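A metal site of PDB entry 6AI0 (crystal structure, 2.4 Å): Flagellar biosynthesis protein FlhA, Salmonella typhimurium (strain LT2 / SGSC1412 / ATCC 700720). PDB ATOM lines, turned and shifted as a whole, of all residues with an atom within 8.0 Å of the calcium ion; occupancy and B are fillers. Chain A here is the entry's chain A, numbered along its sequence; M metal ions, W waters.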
ATOM      1  N   VAL A 257      35.659  -3.484 -17.275  1.00  0.00           N
ATOM      2  CA  VAL A 257      35.591  -3.649 -18.726  1.00  0.00           C
ATOM      3  C   VAL A 257      35.986  -5.070 -19.112  1.00  0.00           C
ATOM      4  O   VAL A 257      35.316  -5.727 -19.919  1.00  0.00           O
ATOM      5  CB  VAL A 257      36.472  -2.608 -19.429  1.00  0.00           C
ATOM      6  CG1 VAL A 257      36.548  -2.893 -20.922  1.00  0.00           C
ATOM      7  CG2 VAL A 257      35.949  -1.203 -19.175  1.00  0.00           C
ATOM      8  N   THR A 264      27.446  -8.091 -18.382  1.00  0.00           N
ATOM      9  CA  THR A 264      26.298  -8.029 -19.286  1.00  0.00           C
ATOM     10  C   THR A 264      25.389  -9.242 -19.108  1.00  0.00           C
ATOM     11  O   THR A 264      24.155  -9.113 -19.160  1.00  0.00           O
ATOM     12  CB  THR A 264      26.781  -7.927 -20.731  1.00  0.00           C
ATOM     13  OG1 THR A 264      27.496  -6.696 -20.914  1.00  0.00           O
ATOM     14  CG2 THR A 264      25.617  -7.989 -21.703  1.00  0.00           C
ATOM     15  N   LEU A 326      22.578   2.864 -17.895  1.00  0.00           N
ATOM     16  CA  LEU A 326      23.714   2.715 -18.806  1.00  0.00           C
ATOM     17  C   LEU A 326      24.134   4.093 -19.300  1.00  0.00           C
ATOM     18  O   LEU A 326      23.325   4.810 -19.901  1.00  0.00           O
ATOM     19  CB  LEU A 326      23.359   1.807 -19.978  1.00  0.00           C
ATOM     20  CG  LEU A 326      24.371   1.802 -21.112  1.00  0.00           C
ATOM     21  CD1 LEU A 326      25.669   1.155 -20.653  1.00  0.00           C
ATOM     22  CD2 LEU A 326      23.821   1.101 -22.339  1.00  0.00           C
ATOM     23  N   SER A 350      28.498   0.737 -17.818  1.00  0.00           N
ATOM     24  CA  SER A 350      29.196   1.591 -18.774  1.00  0.00           C
ATOM     25  C   SER A 350      29.035   1.036 -20.178  1.00  0.00           C
ATOM     26  O   SER A 350      28.887  -0.182 -20.372  1.00  0.00           O
ATOM     27  CB  SER A 350      30.677   1.737 -18.430  1.00  0.00           C
ATOM     28  OG  SER A 350      31.447   1.998 -19.591  1.00  0.00           O
ATOM     29  N   ASN A 351      29.064   1.933 -21.159  1.00  0.00           N
ATOM     30  CA  ASN A 351      28.907   1.498 -22.550  1.00  0.00           C
ATOM     31  C   ASN A 351      30.066   0.614 -22.994  1.00  0.00           C
ATOM     32  O   ASN A 351      29.876  -0.281 -23.817  1.00  0.00           O
ATOM     33  CB  ASN A 351      28.782   2.715 -23.472  1.00  0.00           C
ATOM     34  CG  ASN A 351      30.102   3.416 -23.713  1.00  0.00           C
ATOM     35  OD1 ASN A 351      30.553   4.221 -22.893  1.00  0.00           O
ATOM     36  ND2 ASN A 351      30.734   3.120 -24.842  1.00  0.00           N
ATOM     37  N   LEU A 352      31.263   0.825 -22.444  1.00  0.00           N
ATOM     38  CA  LEU A 352      32.393  -0.039 -22.745  1.00  0.00           C
ATOM     39  C   LEU A 352      32.293  -1.400 -22.050  1.00  0.00           C
ATOM     40  O   LEU A 352      33.037  -2.312 -22.420  1.00  0.00           O
ATOM     41  CB  LEU A 352      33.714   0.627 -22.362  1.00  0.00           C
ATOM     42  CG  LEU A 352      34.076   1.957 -23.037  1.00  0.00           C
ATOM     43  CD1 LEU A 352      35.479   2.382 -22.646  1.00  0.00           C
ATOM     44  CD2 LEU A 352      33.937   1.851 -24.549  1.00  0.00           C
ATOM     45  N   GLU A 353      31.412  -1.543 -21.063  1.00  0.00           N
ATOM     46  CA  GLU A 353      31.212  -2.828 -20.403  1.00  0.00           C
ATOM     47  C   GLU A 353      30.111  -3.653 -21.052  1.00  0.00           C
ATOM     48  O   GLU A 353      30.138  -4.888 -20.977  1.00  0.00           O
ATOM     49  CB  GLU A 353      30.870  -2.626 -18.921  1.00  0.00           C
ATOM     50  CG  GLU A 353      31.862  -1.772 -18.150  1.00  0.00           C
ATOM     51  CD  GLU A 353      31.299  -1.336 -16.807  1.00  0.00           C
ATOM     52  OE1 GLU A 353      30.090  -1.558 -16.572  1.00  0.00           O
ATOM     53  OE2 GLU A 353      32.054  -0.777 -15.995  1.00  0.00           O
ATOM     54  N   LEU A 354      29.122  -2.999 -21.662  1.00  0.00           N
ATOM     55  CA  LEU A 354      28.000  -3.715 -22.263  1.00  0.00           C
ATOM     56  C   LEU A 354      28.435  -4.342 -23.582  1.00  0.00           C
ATOM     57  O   LEU A 354      29.045  -3.680 -24.427  1.00  0.00           O
ATOM     58  CB  LEU A 354      26.823  -2.766 -22.487  1.00  0.00           C
ATOM     59  CG  LEU A 354      25.458  -3.450 -22.607  1.00  0.00           C
ATOM     60  CD1 LEU A 354      25.230  -4.368 -21.424  1.00  0.00           C
ATOM     61  CD2 LEU A 354      24.346  -2.417 -22.697  1.00  0.00           C
ATOM     62  N   SER A 355      28.111  -5.621 -23.758  1.00  0.00           N
ATOM     63  CA  SER A 355      28.500  -6.352 -24.951  1.00  0.00           C
ATOM     64  C   SER A 355      27.905  -5.697 -26.199  1.00  0.00           C
ATOM     65  O   SER A 355      26.687  -5.511 -26.295  1.00  0.00           O
ATOM     66  CB  SER A 355      28.055  -7.803 -24.837  1.00  0.00           C
ATOM     67  OG  SER A 355      28.414  -8.350 -23.584  1.00  0.00           O
ATOM     68  N   ASP A 356      28.787  -5.344 -27.143  1.00  0.00           N
ATOM     69  CA  ASP A 356      28.387  -4.665 -28.376  1.00  0.00           C
ATOM     70  C   ASP A 356      27.593  -5.557 -29.322  1.00  0.00           C
ATOM     71  O   ASP A 356      27.253  -5.110 -30.420  1.00  0.00           O
ATOM     72  CB  ASP A 356      29.620  -4.126 -29.087  1.00  0.00           C
ATOM     73  CG  ASP A 356      30.234  -2.949 -28.370  1.00  0.00           C
ATOM     74  OD1 ASP A 356      29.612  -2.476 -27.407  1.00  0.00           O
ATOM     75  OD2 ASP A 356      31.335  -2.514 -28.764  1.00  0.00           O
ATOM     76  N   ASN A 357      27.276  -6.793 -28.923  1.00  0.00           N
ATOM     77  CA  ASN A 357      26.550  -7.720 -29.772  1.00  0.00           C
ATOM     78  C   ASN A 357      25.098  -7.879 -29.362  1.00  0.00           C
ATOM     79  O   ASN A 357      24.400  -8.763 -29.887  1.00  0.00           O
ATOM     80  CB  ASN A 357      27.240  -9.084 -29.774  1.00  0.00           C
ATOM     81  CG  ASN A 357      26.909  -9.902 -28.541  1.00  0.00           C
ATOM     82  OD1 ASN A 357      27.352  -9.593 -27.431  1.00  0.00           O
ATOM     83  ND2 ASN A 357      26.117 -10.957 -28.724  1.00  0.00           N
ATOM     84  N   ILE A 360      19.895  -2.994 -27.647  1.00  0.00           N
ATOM     85  CA  ILE A 360      19.679  -2.149 -26.483  1.00  0.00           C
ATOM     86  C   ILE A 360      18.534  -1.194 -26.785  1.00  0.00           C
ATOM     87  O   ILE A 360      18.581  -0.447 -27.774  1.00  0.00           O
ATOM     88  CB  ILE A 360      20.948  -1.371 -26.096  1.00  0.00           C
ATOM     89  CG1 ILE A 360      22.114  -2.335 -25.920  1.00  0.00           C
ATOM     90  CG2 ILE A 360      20.723  -0.539 -24.850  1.00  0.00           C
ATOM     91  CD1 ILE A 360      23.476  -1.701 -26.122  1.00  0.00           C
HETATM   92 CA    CA M   1      30.483  -1.700 -25.470  1.00  0.00          CA
HETATM   93  O   HOH W   1      29.957   1.366 -26.570  1.00  0.00           O
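OG of Ser 350 lies within hydrogen-bond range of N of Leu 352 (3.1 Å).
Residues that only touch the calcium ion: Leu 352 (3.7 Å).
Of the 12 residues printed, 4 come within 4 Å of the calcium ion.
The calcium ion is bound by O of Asn 351 (2.3 Å), OD1 of Asp 356 (2.3 Å) and O of Leu 354 (2.7 Å).
The calcium ion has three donor atoms within binding distance.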
